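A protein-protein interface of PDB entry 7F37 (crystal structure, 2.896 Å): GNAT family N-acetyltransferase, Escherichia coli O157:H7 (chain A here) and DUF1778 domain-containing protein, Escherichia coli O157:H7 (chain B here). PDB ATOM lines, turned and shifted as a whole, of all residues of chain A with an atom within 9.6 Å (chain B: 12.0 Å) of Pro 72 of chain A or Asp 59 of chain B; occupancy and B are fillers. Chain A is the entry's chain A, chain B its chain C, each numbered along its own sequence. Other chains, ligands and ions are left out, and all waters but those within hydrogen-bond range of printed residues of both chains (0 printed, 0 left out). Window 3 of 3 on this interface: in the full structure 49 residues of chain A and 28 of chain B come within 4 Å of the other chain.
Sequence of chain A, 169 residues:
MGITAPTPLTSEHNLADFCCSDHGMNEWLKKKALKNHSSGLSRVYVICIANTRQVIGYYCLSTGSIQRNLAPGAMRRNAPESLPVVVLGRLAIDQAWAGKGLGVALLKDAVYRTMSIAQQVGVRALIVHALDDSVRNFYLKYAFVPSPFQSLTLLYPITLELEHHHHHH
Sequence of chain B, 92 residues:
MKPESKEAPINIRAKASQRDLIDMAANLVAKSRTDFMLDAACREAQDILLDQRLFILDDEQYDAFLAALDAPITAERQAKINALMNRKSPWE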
ATOM      1  N   GLN A  67     -20.841  -0.113  33.979  1.00  0.00           N
ATOM      2  CA  GLN A  67     -19.916  -1.218  34.220  1.00  0.00           C
ATOM      3  C   GLN A  67     -19.991  -2.283  33.139  1.00  0.00           C
ATOM      4  O   GLN A  67     -21.070  -2.591  32.634  1.00  0.00           O
ATOM      5  CB  GLN A  67     -20.180  -1.866  35.579  1.00  0.00           C
ATOM      6  CG  GLN A  67     -20.020  -0.871  36.707  1.00  0.00           C
ATOM      7  CD  GLN A  67     -19.302  -1.434  37.891  1.00  0.00           C
ATOM      8  OE1 GLN A  67     -18.409  -2.282  37.764  1.00  0.00           O
ATOM      9  NE2 GLN A  67     -19.648  -0.932  39.060  1.00  0.00           N
ATOM     10  N   ARG A  68     -18.826  -2.836  32.800  1.00  0.00           N
ATOM     11  CA  ARG A  68     -18.713  -3.982  31.911  1.00  0.00           C
ATOM     12  C   ARG A  68     -19.049  -5.248  32.675  1.00  0.00           C
ATOM     13  O   ARG A  68     -18.352  -5.595  33.637  1.00  0.00           O
ATOM     14  CB  ARG A  68     -17.298  -4.093  31.351  1.00  0.00           C
ATOM     15  CG  ARG A  68     -17.137  -3.646  29.909  1.00  0.00           C
ATOM     16  CD  ARG A  68     -15.814  -4.147  29.308  1.00  0.00           C
ATOM     17  NE  ARG A  68     -15.472  -3.540  28.017  1.00  0.00           N
ATOM     18  CZ  ARG A  68     -16.160  -3.754  26.900  1.00  0.00           C
ATOM     19  NH1 ARG A  68     -15.787  -3.202  25.747  1.00  0.00           N
ATOM     20  NH2 ARG A  68     -17.239  -4.527  26.940  1.00  0.00           N
ATOM     21  N   ASN A  69     -20.096  -5.940  32.238  1.00  0.00           N
ATOM     22  CA  ASN A  69     -20.427  -7.264  32.753  1.00  0.00           C
ATOM     23  C   ASN A  69     -19.209  -8.178  32.767  1.00  0.00           C
ATOM     24  O   ASN A  69     -18.676  -8.524  31.714  1.00  0.00           O
ATOM     25  CB  ASN A  69     -21.518  -7.877  31.878  1.00  0.00           C
ATOM     26  CG  ASN A  69     -22.259  -8.966  32.573  1.00  0.00           C
ATOM     27  OD1 ASN A  69     -21.983  -9.285  33.724  1.00  0.00           O
ATOM     28  ND2 ASN A  69     -23.221  -9.547  31.884  1.00  0.00           N
ATOM     29  N   LEU A  70     -18.782  -8.594  33.963  1.00  0.00           N
ATOM     30  CA  LEU A  70     -17.664  -9.527  34.061  1.00  0.00           C
ATOM     31  C   LEU A  70     -17.947 -10.825  33.330  1.00  0.00           C
ATOM     32  O   LEU A  70     -17.017 -11.529  32.932  1.00  0.00           O
ATOM     33  CB  LEU A  70     -17.344  -9.840  35.515  1.00  0.00           C
ATOM     34  CG  LEU A  70     -16.802  -8.642  36.275  1.00  0.00           C
ATOM     35  CD1 LEU A  70     -16.426  -9.054  37.694  1.00  0.00           C
ATOM     36  CD2 LEU A  70     -15.626  -8.045  35.516  1.00  0.00           C
ATOM     37  N   ALA A  71     -19.213 -11.171  33.165  1.00  0.00           N
ATOM     38  CA  ALA A  71     -19.604 -12.414  32.522  1.00  0.00           C
ATOM     39  C   ALA A  71     -20.741 -12.104  31.567  1.00  0.00           C
ATOM     40  O   ALA A  71     -21.912 -12.288  31.923  1.00  0.00           O
ATOM     41  CB  ALA A  71     -20.033 -13.455  33.555  1.00  0.00           C
ATOM     42  N   PRO A  72     -20.441 -11.624  30.347  1.00  0.00           N
ATOM     43  CA  PRO A  72     -21.515 -11.524  29.332  1.00  0.00           C
ATOM     44  C   PRO A  72     -22.130 -12.883  29.033  1.00  0.00           C
ATOM     45  O   PRO A  72     -23.318 -12.973  28.690  1.00  0.00           O
ATOM     46  CB  PRO A  72     -20.812 -10.908  28.106  1.00  0.00           C
ATOM     47  CG  PRO A  72     -19.481 -10.416  28.595  1.00  0.00           C
ATOM     48  CD  PRO A  72     -19.123 -11.249  29.804  1.00  0.00           C
ATOM     49  N   GLY A  73     -21.323 -13.947  29.148  1.00  0.00           N
ATOM     50  CA  GLY A  73     -21.756 -15.328  29.295  1.00  0.00           C
ATOM     51  C   GLY A  73     -20.661 -16.154  29.953  1.00  0.00           C
ATOM     52  O   GLY A  73     -19.481 -15.923  29.680  1.00  0.00           O
ATOM     53  N   ALA A  74     -21.026 -17.063  30.859  1.00  0.00           N
ATOM     54  CA  ALA A  74     -20.125 -18.082  31.429  1.00  0.00           C
ATOM     55  C   ALA A  74     -18.711 -17.562  31.715  1.00  0.00           C
ATOM     56  O   ALA A  74     -17.711 -18.231  31.435  1.00  0.00           O
ATOM     57  CB  ALA A  74     -20.058 -19.308  30.517  1.00  0.00           C
ATOM     58  N   MET A  75     -18.640 -16.352  32.283  1.00  0.00           N
ATOM     59  CA  MET A  75     -17.408 -15.769  32.831  1.00  0.00           C
ATOM     60  C   MET A  75     -16.281 -15.621  31.786  1.00  0.00           C
ATOM     61  O   MET A  75     -15.148 -16.060  32.009  1.00  0.00           O
ATOM     62  CB  MET A  75     -16.936 -16.599  34.038  1.00  0.00           C
ATOM     63  CG  MET A  75     -17.488 -16.199  35.425  1.00  0.00           C
ATOM     64  SD  MET A  75     -19.286 -16.145  35.643  1.00  0.00           S
ATOM     65  CE  MET A  75     -19.629 -17.737  36.394  1.00  0.00           C
ATOM     66  N   ARG A  76     -16.584 -14.933  30.659  1.00  0.00           N
ATOM     67  CA  ARG A  76     -15.654 -14.758  29.534  1.00  0.00           C
ATOM     68  C   ARG A  76     -14.715 -13.554  29.725  1.00  0.00           C
ATOM     69  O   ARG A  76     -14.568 -13.035  30.837  1.00  0.00           O
ATOM     70  CB  ARG A  76     -16.402 -14.655  28.192  1.00  0.00           C
ATOM     71  CG  ARG A  76     -17.008 -15.962  27.682  1.00  0.00           C
ATOM     72  CD  ARG A  76     -18.377 -15.766  27.021  1.00  0.00           C
ATOM     73  NE  ARG A  76     -18.316 -15.186  25.682  1.00  0.00           N
ATOM     74  CZ  ARG A  76     -19.265 -14.413  25.163  1.00  0.00           C
ATOM     75  NH1 ARG A  76     -20.326 -14.104  25.893  1.00  0.00           N
ATOM     76  NH2 ARG A  76     -19.143 -13.929  23.930  1.00  0.00           N
ATOM     77  N   ARG A  77     -14.051 -13.119  28.631  1.00  0.00           N
ATOM     78  CA  ARG A  77     -12.916 -12.174  28.672  1.00  0.00           C
ATOM     79  C   ARG A  77     -13.402 -10.748  28.944  1.00  0.00           C
ATOM     80  O   ARG A  77     -13.313  -9.842  28.104  1.00  0.00           O
ATOM     81  CB  ARG A  77     -12.094 -12.228  27.381  1.00  0.00           C
ATOM     82  CG  ARG A  77     -10.848 -11.275  27.338  1.00  0.00           C
ATOM     83  CD  ARG A  77     -10.003 -11.412  26.048  1.00  0.00           C
ATOM     84  NE  ARG A  77     -10.705 -11.005  24.822  1.00  0.00           N
ATOM     85  CZ  ARG A  77     -10.809  -9.748  24.395  1.00  0.00           C
ATOM     86  NH1 ARG A  77     -11.454  -9.455  23.266  1.00  0.00           N
ATOM     87  NH2 ARG A  77     -10.269  -8.774  25.103  1.00  0.00           N
ATOM     88  N   ASN A  78     -13.893 -10.553  30.168  1.00  0.00           N
ATOM     89  CA  ASN A  78     -14.204  -9.232  30.694  1.00  0.00           C
ATOM     90  C   ASN A  78     -13.615  -9.165  32.092  1.00  0.00           C
ATOM     91  O   ASN A  78     -13.868 -10.048  32.913  1.00  0.00           O
ATOM     92  CB  ASN A  78     -15.717  -8.956  30.694  1.00  0.00           C
ATOM     93  CG  ASN A  78     -16.187  -8.215  29.416  1.00  0.00           C
ATOM     94  OD1 ASN A  78     -15.403  -7.981  28.490  1.00  0.00           O
ATOM     95  ND2 ASN A  78     -17.469  -7.857  29.366  1.00  0.00           N
ATOM     96  N   ALA A  79     -12.745  -8.129  32.338  1.00  0.00           N
ATOM     97  CA  ALA A  79     -12.091  -7.696  33.563  1.00  0.00           C
ATOM     98  C   ALA A  79     -12.850  -6.527  34.167  1.00  0.00           C
ATOM     99  O   ALA A  79     -13.576  -5.819  33.462  1.00  0.00           O
ATOM    100  CB  ALA A  79     -10.646  -7.271  33.300  1.00  0.00           C
ATOM    101  N   GLU A  81     -14.211  -3.311  34.905  1.00  0.00           N
ATOM    102  CA  GLU A  81     -14.073  -2.040  34.206  1.00  0.00           C
ATOM    103  C   GLU A  81     -15.302  -1.200  34.485  1.00  0.00           C
ATOM    104  O   GLU A  81     -16.419  -1.598  34.140  1.00  0.00           O
ATOM    105  CB  GLU A  81     -13.909  -2.245  32.708  1.00  0.00           C
ATOM    106  CG  GLU A  81     -13.541  -0.995  31.938  1.00  0.00           C
ATOM    107  CD  GLU A  81     -13.326  -1.325  30.486  1.00  0.00           C
ATOM    108  OE1 GLU A  81     -13.206  -0.413  29.635  1.00  0.00           O
ATOM    109  OE2 GLU A  81     -13.284  -2.536  30.198  1.00  0.00           O
ATOM    110  N   PRO A 148     -27.125   4.572  24.018  1.00  0.00           N
ATOM    111  CA  PRO A 148     -27.225   3.352  23.214  1.00  0.00           C
ATOM    112  C   PRO A 148     -27.778   2.193  23.991  1.00  0.00           C
ATOM    113  O   PRO A 148     -28.324   1.269  23.378  1.00  0.00           O
ATOM    114  CB  PRO A 148     -25.781   3.083  22.810  1.00  0.00           C
ATOM    115  CG  PRO A 148     -25.034   3.517  24.005  1.00  0.00           C
ATOM    116  CD  PRO A 148     -25.785   4.714  24.600  1.00  0.00           C
ATOM    117  N   PHE A 149     -27.668   2.222  25.325  1.00  0.00           N
ATOM    118  CA  PHE A 149     -27.942   1.056  26.156  1.00  0.00           C
ATOM    119  C   PHE A 149     -29.357   1.007  26.717  1.00  0.00           C
ATOM    120  O   PHE A 149     -29.760  -0.054  27.200  1.00  0.00           O
ATOM    121  CB  PHE A 149     -26.939   0.958  27.322  1.00  0.00           C
ATOM    122  CG  PHE A 149     -26.904   2.170  28.222  1.00  0.00           C
ATOM    123  CD1 PHE A 149     -25.868   3.097  28.118  1.00  0.00           C
ATOM    124  CD2 PHE A 149     -27.892   2.379  29.184  1.00  0.00           C
ATOM    125  CE1 PHE A 149     -25.826   4.210  28.949  1.00  0.00           C
ATOM    126  CE2 PHE A 149     -27.862   3.498  30.017  1.00  0.00           C
ATOM    127  CZ  PHE A 149     -26.829   4.410  29.906  1.00  0.00           C
ATOM    128  N   PHE B  55     -25.688   0.792  35.977  1.00  0.00           N
ATOM    129  CA  PHE B  55     -25.972   0.193  34.681  1.00  0.00           C
ATOM    130  C   PHE B  55     -24.876  -0.817  34.419  1.00  0.00           C
ATOM    131  O   PHE B  55     -23.732  -0.441  34.150  1.00  0.00           O
ATOM    132  CB  PHE B  55     -26.001   1.218  33.559  1.00  0.00           C
ATOM    133  CG  PHE B  55     -26.714   2.473  33.906  1.00  0.00           C
ATOM    134  CD1 PHE B  55     -26.081   3.463  34.642  1.00  0.00           C
ATOM    135  CD2 PHE B  55     -28.009   2.688  33.478  1.00  0.00           C
ATOM    136  CE1 PHE B  55     -26.724   4.638  34.959  1.00  0.00           C
ATOM    137  CE2 PHE B  55     -28.666   3.869  33.795  1.00  0.00           C
ATOM    138  CZ  PHE B  55     -28.022   4.843  34.541  1.00  0.00           C
ATOM    139  N   ILE B  56     -25.218  -2.091  34.498  1.00  0.00           N
ATOM    140  CA  ILE B  56     -24.295  -3.156  34.157  1.00  0.00           C
ATOM    141  C   ILE B  56     -24.664  -3.600  32.750  1.00  0.00           C
ATOM    142  O   ILE B  56     -25.696  -4.238  32.532  1.00  0.00           O
ATOM    143  CB  ILE B  56     -24.361  -4.290  35.168  1.00  0.00           C
ATOM    144  CG1 ILE B  56     -24.041  -3.737  36.546  1.00  0.00           C
ATOM    145  CG2 ILE B  56     -23.367  -5.355  34.821  1.00  0.00           C
ATOM    146  CD1 ILE B  56     -24.146  -4.754  37.632  1.00  0.00           C
ATOM    147  N   LEU B  57     -23.841  -3.222  31.785  1.00  0.00           N
ATOM    148  CA  LEU B  57     -24.109  -3.444  30.376  1.00  0.00           C
ATOM    149  C   LEU B  57     -23.175  -4.508  29.830  1.00  0.00           C
ATOM    150  O   LEU B  57     -22.186  -4.881  30.466  1.00  0.00           O
ATOM    151  CB  LEU B  57     -23.934  -2.154  29.582  1.00  0.00           C
ATOM    152  CG  LEU B  57     -24.417  -0.954  30.360  1.00  0.00           C
ATOM    153  CD1 LEU B  57     -23.845   0.288  29.737  1.00  0.00           C
ATOM    154  CD2 LEU B  57     -25.941  -0.958  30.341  1.00  0.00           C
ATOM    155  N   ASP B  58     -23.520  -5.004  28.642  1.00  0.00           N
ATOM    156  CA  ASP B  58     -22.736  -6.014  27.968  1.00  0.00           C
ATOM    157  C   ASP B  58     -21.743  -5.330  27.032  1.00  0.00           C
ATOM    158  O   ASP B  58     -21.701  -4.103  26.910  1.00  0.00           O
ATOM    159  CB  ASP B  58     -23.641  -7.006  27.227  1.00  0.00           C
ATOM    160  CG  ASP B  58     -24.052  -6.523  25.811  1.00  0.00           C
ATOM    161  OD1 ASP B  58     -24.470  -7.374  24.982  1.00  0.00           O
ATOM    162  OD2 ASP B  58     -23.992  -5.308  25.524  1.00  0.00           O
ATOM    163  N   ASP B  59     -20.967  -6.146  26.321  1.00  0.00           N
ATOM    164  CA  ASP B  59     -19.889  -5.617  25.497  1.00  0.00           C
ATOM    165  C   ASP B  59     -20.421  -4.755  24.354  1.00  0.00           C
ATOM    166  O   ASP B  59     -20.060  -3.580  24.238  1.00  0.00           O
ATOM    167  CB  ASP B  59     -19.035  -6.768  24.988  1.00  0.00           C
ATOM    168  CG  ASP B  59     -18.474  -7.584  26.113  1.00  0.00           C
ATOM    169  OD1 ASP B  59     -17.423  -7.221  26.682  1.00  0.00           O
ATOM    170  OD2 ASP B  59     -19.141  -8.571  26.469  1.00  0.00           O
ATOM    171  N   GLU B  60     -21.273  -5.315  23.490  1.00  0.00           N
ATOM    172  CA  GLU B  60     -21.804  -4.494  22.405  1.00  0.00           C
ATOM    173  C   GLU B  60     -22.363  -3.177  22.941  1.00  0.00           C
ATOM    174  O   GLU B  60     -22.246  -2.130  22.285  1.00  0.00           O
ATOM    175  CB  GLU B  60     -22.876  -5.268  21.614  1.00  0.00           C
ATOM    176  CG  GLU B  60     -23.836  -4.367  20.792  1.00  0.00           C
ATOM    177  CD  GLU B  60     -24.512  -5.074  19.599  1.00  0.00           C
ATOM    178  OE1 GLU B  60     -24.896  -6.254  19.746  1.00  0.00           O
ATOM    179  OE2 GLU B  60     -24.685  -4.443  18.523  1.00  0.00           O
ATOM    180  N   GLN B  61     -22.911  -3.201  24.161  1.00  0.00           N
ATOM    181  CA  GLN B  61     -23.545  -2.013  24.714  1.00  0.00           C
ATOM    182  C   GLN B  61     -22.553  -1.083  25.385  1.00  0.00           C
ATOM    183  O   GLN B  61     -22.717   0.138  25.316  1.00  0.00           O
ATOM    184  CB  GLN B  61     -24.617  -2.402  25.724  1.00  0.00           C
ATOM    185  CG  GLN B  61     -26.000  -2.542  25.150  1.00  0.00           C
ATOM    186  CD  GLN B  61     -26.994  -2.998  26.196  1.00  0.00           C
ATOM    187  OE1 GLN B  61     -26.627  -3.325  27.330  1.00  0.00           O
ATOM    188  NE2 GLN B  61     -28.263  -3.019  25.821  1.00  0.00           N
ATOM    189  N   TYR B  62     -21.539  -1.630  26.056  1.00  0.00           N
ATOM    190  CA  TYR B  62     -20.573  -0.781  26.746  1.00  0.00           C
ATOM    191  C   TYR B  62     -19.639  -0.092  25.748  1.00  0.00           C
ATOM    192  O   TYR B  62     -19.323   1.090  25.913  1.00  0.00           O
ATOM    193  CB  TYR B  62     -19.796  -1.613  27.776  1.00  0.00           C
ATOM    194  CG  TYR B  62     -18.933  -0.809  28.732  1.00  0.00           C
ATOM    195  CD1 TYR B  62     -19.407  -0.432  29.980  1.00  0.00           C
ATOM    196  CD2 TYR B  62     -17.636  -0.439  28.394  1.00  0.00           C
ATOM    197  CE1 TYR B  62     -18.619   0.310  30.857  1.00  0.00           C
ATOM    198  CE2 TYR B  62     -16.845   0.300  29.263  1.00  0.00           C
ATOM    199  CZ  TYR B  62     -17.347   0.673  30.488  1.00  0.00           C
ATOM    200  OH  TYR B  62     -16.582   1.413  31.352  1.00  0.00           O
ATOM    201  N   ASP B  63     -19.207  -0.802  24.697  1.00  0.00           N
ATOM    202  CA  ASP B  63     -18.516  -0.145  23.588  1.00  0.00           C
ATOM    203  C   ASP B  63     -19.408   0.902  22.927  1.00  0.00           C
ATOM    204  O   ASP B  63     -19.013   2.062  22.769  1.00  0.00           O
ATOM    205  CB  ASP B  63     -18.071  -1.186  22.575  1.00  0.00           C
ATOM    206  CG  ASP B  63     -16.996  -2.080  23.120  1.00  0.00           C
ATOM    207  OD1 ASP B  63     -16.160  -1.568  23.900  1.00  0.00           O
ATOM    208  OD2 ASP B  63     -16.972  -3.301  22.801  1.00  0.00           O
ATOM    209  N   ALA B  64     -20.639   0.519  22.573  1.00  0.00           N
ATOM    210  CA  ALA B  64     -21.590   1.476  22.016  1.00  0.00           C
ATOM    211  C   ALA B  64     -21.753   2.694  22.906  1.00  0.00           C
ATOM    212  O   ALA B  64     -22.150   3.762  22.430  1.00  0.00           O
ATOM    213  CB  ALA B  64     -22.942   0.799  21.793  1.00  0.00           C
ATOM    214  N   PHE B  65     -21.472   2.544  24.201  1.00  0.00           N
ATOM    215  CA  PHE B  65     -21.401   3.680  25.110  1.00  0.00           C
ATOM    216  C   PHE B  65     -20.061   4.401  24.990  1.00  0.00           C
ATOM    217  O   PHE B  65     -20.023   5.619  24.789  1.00  0.00           O
ATOM    218  CB  PHE B  65     -21.635   3.203  26.541  1.00  0.00           C
ATOM    219  CG  PHE B  65     -21.355   4.243  27.592  1.00  0.00           C
ATOM    220  CD1 PHE B  65     -22.194   5.340  27.749  1.00  0.00           C
ATOM    221  CD2 PHE B  65     -20.268   4.109  28.445  1.00  0.00           C
ATOM    222  CE1 PHE B  65     -21.938   6.293  28.722  1.00  0.00           C
ATOM    223  CE2 PHE B  65     -20.009   5.057  29.422  1.00  0.00           C
ATOM    224  CZ  PHE B  65     -20.847   6.150  29.560  1.00  0.00           C
ATOM    225  N   LEU B  66     -18.951   3.662  25.104  1.00  0.00           N
ATOM    226  CA  LEU B  66     -17.643   4.271  24.890  1.00  0.00           C
ATOM    227  C   LEU B  66     -17.599   5.023  23.568  1.00  0.00           C
ATOM    228  O   LEU B  66     -17.036   6.122  23.489  1.00  0.00           O
ATOM    229  CB  LEU B  66     -16.538   3.219  24.920  1.00  0.00           C
ATOM    230  CG  LEU B  66     -16.367   2.271  26.094  1.00  0.00           C
ATOM    231  CD1 LEU B  66     -15.560   1.063  25.625  1.00  0.00           C
ATOM    232  CD2 LEU B  66     -15.684   2.953  27.260  1.00  0.00           C
ATOM    233  N   ALA B  67     -18.183   4.441  22.518  1.00  0.00           N
ATOM    234  CA  ALA B  67     -18.376   5.175  21.278  1.00  0.00           C
ATOM    235  C   ALA B  67     -18.972   6.531  21.573  1.00  0.00           C
ATOM    236  O   ALA B  67     -18.391   7.568  21.247  1.00  0.00           O
ATOM    237  CB  ALA B  67     -19.291   4.398  20.339  1.00  0.00           C
ATOM    238  N   ALA B  68     -20.111   6.537  22.257  1.00  0.00           N
ATOM    239  CA  ALA B  68     -20.842   7.782  22.450  1.00  0.00           C
ATOM    240  C   ALA B  68     -19.973   8.852  23.107  1.00  0.00           C
ATOM    241  O   ALA B  68     -20.146  10.044  22.833  1.00  0.00           O
ATOM    242  CB  ALA B  68     -22.103   7.520  23.271  1.00  0.00           C
ATOM    243  N   LEU B  69     -19.019   8.456  23.947  1.00  0.00           N
ATOM    244  CA  LEU B  69     -18.175   9.451  24.590  1.00  0.00           C
ATOM    245  C   LEU B  69     -16.986   9.825  23.724  1.00  0.00           C
ATOM    246  O   LEU B  69     -16.491  10.955  23.813  1.00  0.00           O
ATOM    247  CB  LEU B  69     -17.683   8.937  25.933  1.00  0.00           C
ATOM    248  CG  LEU B  69     -18.752   8.760  27.001  1.00  0.00           C
ATOM    249  CD1 LEU B  69     -18.425   7.521  27.790  1.00  0.00           C
ATOM    250  CD2 LEU B  69     -18.827   9.979  27.912  1.00  0.00           C
ATOM    251  N   ASP B  70     -16.499   8.884  22.912  1.00  0.00           N
ATOM    252  CA  ASP B  70     -15.470   9.179  21.916  1.00  0.00           C
ATOM    253  C   ASP B  70     -16.178   9.585  20.626  1.00  0.00           C
ATOM    254  O   ASP B  70     -16.358   8.802  19.691  1.00  0.00           O
ATOM    255  CB  ASP B  70     -14.528   7.993  21.707  1.00  0.00           C
ATOM    256  CG  ASP B  70     -13.955   7.449  23.013  1.00  0.00           C
ATOM    257  OD1 ASP B  70     -13.692   8.275  23.927  1.00  0.00           O
ATOM    258  OD2 ASP B  70     -13.728   6.211  23.113  1.00  0.00           O
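Of chain B, only Leu 57, Asp 59, Tyr 62 and Asp 63 come within 4 Å of Arg 68 of chain A. Asn 69 of chain A touches just one residue of chain B: Leu 57. No residue of chain B comes within 4 Å of Ala 71 of chain A. Pro 72 of chain A touches just one residue of chain B: Asp 59 (2.8 Å). No residue of chain B comes within 4 Å of Ala 74 of chain A. No residue of chain B comes within 4 Å of Arg 76 of chain A. Asn 78 of chain A touches one residue of chain B. Printed residues of chain B within 4 Å of Pro 148 of chain A: Ala 64 and Phe 65. Asp 59 of chain B touches three residues of chain A. Of the printed residues of chain A, Tyr 62 of chain B touches Gln 67 (3.7 Å), Arg 68 (3.6 Å) and Glu 81 (3.7 Å). Of the printed residues of chain A, Ala 64 of chain B touches Pro 148. Ala 68 of chain B touches none of the printed residues of chain A. Asp 70 of chain B touches none of the printed residues of chain A. The nearest residue of chain B that does not touch Pro 72 of chain A is Asp 58 of chain B (4.9 Å). The nearest residue of chain A that does not touch Asp 59 of chain B is Arg 77 of chain A (5.1 Å). The nearest printed residue of chain A that does not touch Ile 56 of chain B is Asn 69 of chain A (4.1 Å).
The backbone NH of Gln 67 of chain A lies within hydrogen-bond range of the backbone carbonyl oxygen of Phe 55 of chain B (2.9 Å). The backbone carbonyl oxygen (O) of Gln 67 of chain A is in hydrogen-bond range of the backbone NH (N) of Leu 57 of chain B, 3.0 Å away. The guanidinium group (NH2) of Arg 68 of chain A lies within salt-bridge range of the side-chain carboxylate (OD1) of Asp 59 of chain B, 2.7 Å away. NH1 of Arg 68 of chain A lies within salt-bridge range of OD1 of Asp 63 of chain B (2.5 Å). N of Asn 69 of chain A lies within hydrogen-bond range of O of Leu 57 of chain B, 2.9 Å away. The side-chain amide nitrogen (ND2) of Asn 78 of chain A lies within hydrogen-bond range of the side-chain carboxylate (OD1) of Asp 59 of chain B (2.8 Å).
Of the 16 printed residues of chain A, 8 touch a printed residue of chain B. Printed residues of chain A that touch a printed residue of chain B: Gln 67, Arg 68, Asn 69, Pro 72, Asn 78, Glu 81, Pro 148 and Phe 149. Hydrophobic or aromatic side chains of chain A that line the printed part of chain B: Pro 72, Pro 148 and Phe 149. Of the 16 printed residues of chain B, 9 touch a printed residue of chain A. Hydrophobic or aromatic side chains of chain B within 4 Å of the printed part of chain A: Phe 55, Leu 57, Tyr 62, Ala 64 and Phe 65. Among the printed residues, Asp or Glu carboxylates within 4 Å of a Lys or Arg side-chain nitrogen of the other chain: Arg 68 of chain A with Asp 59 of chain B (2.7 Å) and Arg 68 of chain A with Asp 63 of chain B (2.5 Å).
Among the printed residues, pairs that only touch across the chains: Gln 67 of chain A with Ile 56 of chain B (3.6 Å), Gln 67 of chain A with Tyr 62 of chain B (3.7 Å), Arg 68 of chain A with Leu 57 of chain B (3.9 Å), Arg 68 of chain A with Tyr 62 of chain B (3.6 Å), Pro 72 of chain A with Asp 59 of chain B (2.8 Å), Glu 81 of chain A with Tyr 62 of chain B (3.7 Å), Pro 148 of chain A with Ala 64 of chain B (3.3 Å), Pro 148 of chain A with Phe 65 of chain B (3.7 Å), Phe 149 of chain A with Phe 55 of chain B (3.6 Å), Phe 149 of chain A with Leu 57 of chain B (3.7 Å), Phe 149 of chain A with Gln 61 of chain B (3.6 Å) and Phe 149 of chain A with Phe 65 of chain B (3.99 Å).
The guanidinium group of Arg 68 of chain A lies within salt-bridge range of the side-chain carboxylate of Glu 81 of chain A (3.2 Å). The side-chain amide nitrogen of Asn 69 of chain A sits at hydrogen-bond distance from the backbone carbonyl oxygen of Ala 71 of chain A (3.0 Å). The side-chain amide nitrogen (ND2) of Asn 78 of chain A is in hydrogen-bond range of the backbone carbonyl oxygen (O) of Asn 69 of chain A (2.7 Å). The side-chain carboxylate (OD2) of Asp 58 of chain B lies within hydrogen-bond range of the backbone NH (N) of Gln 61 of chain B (2.7 Å).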
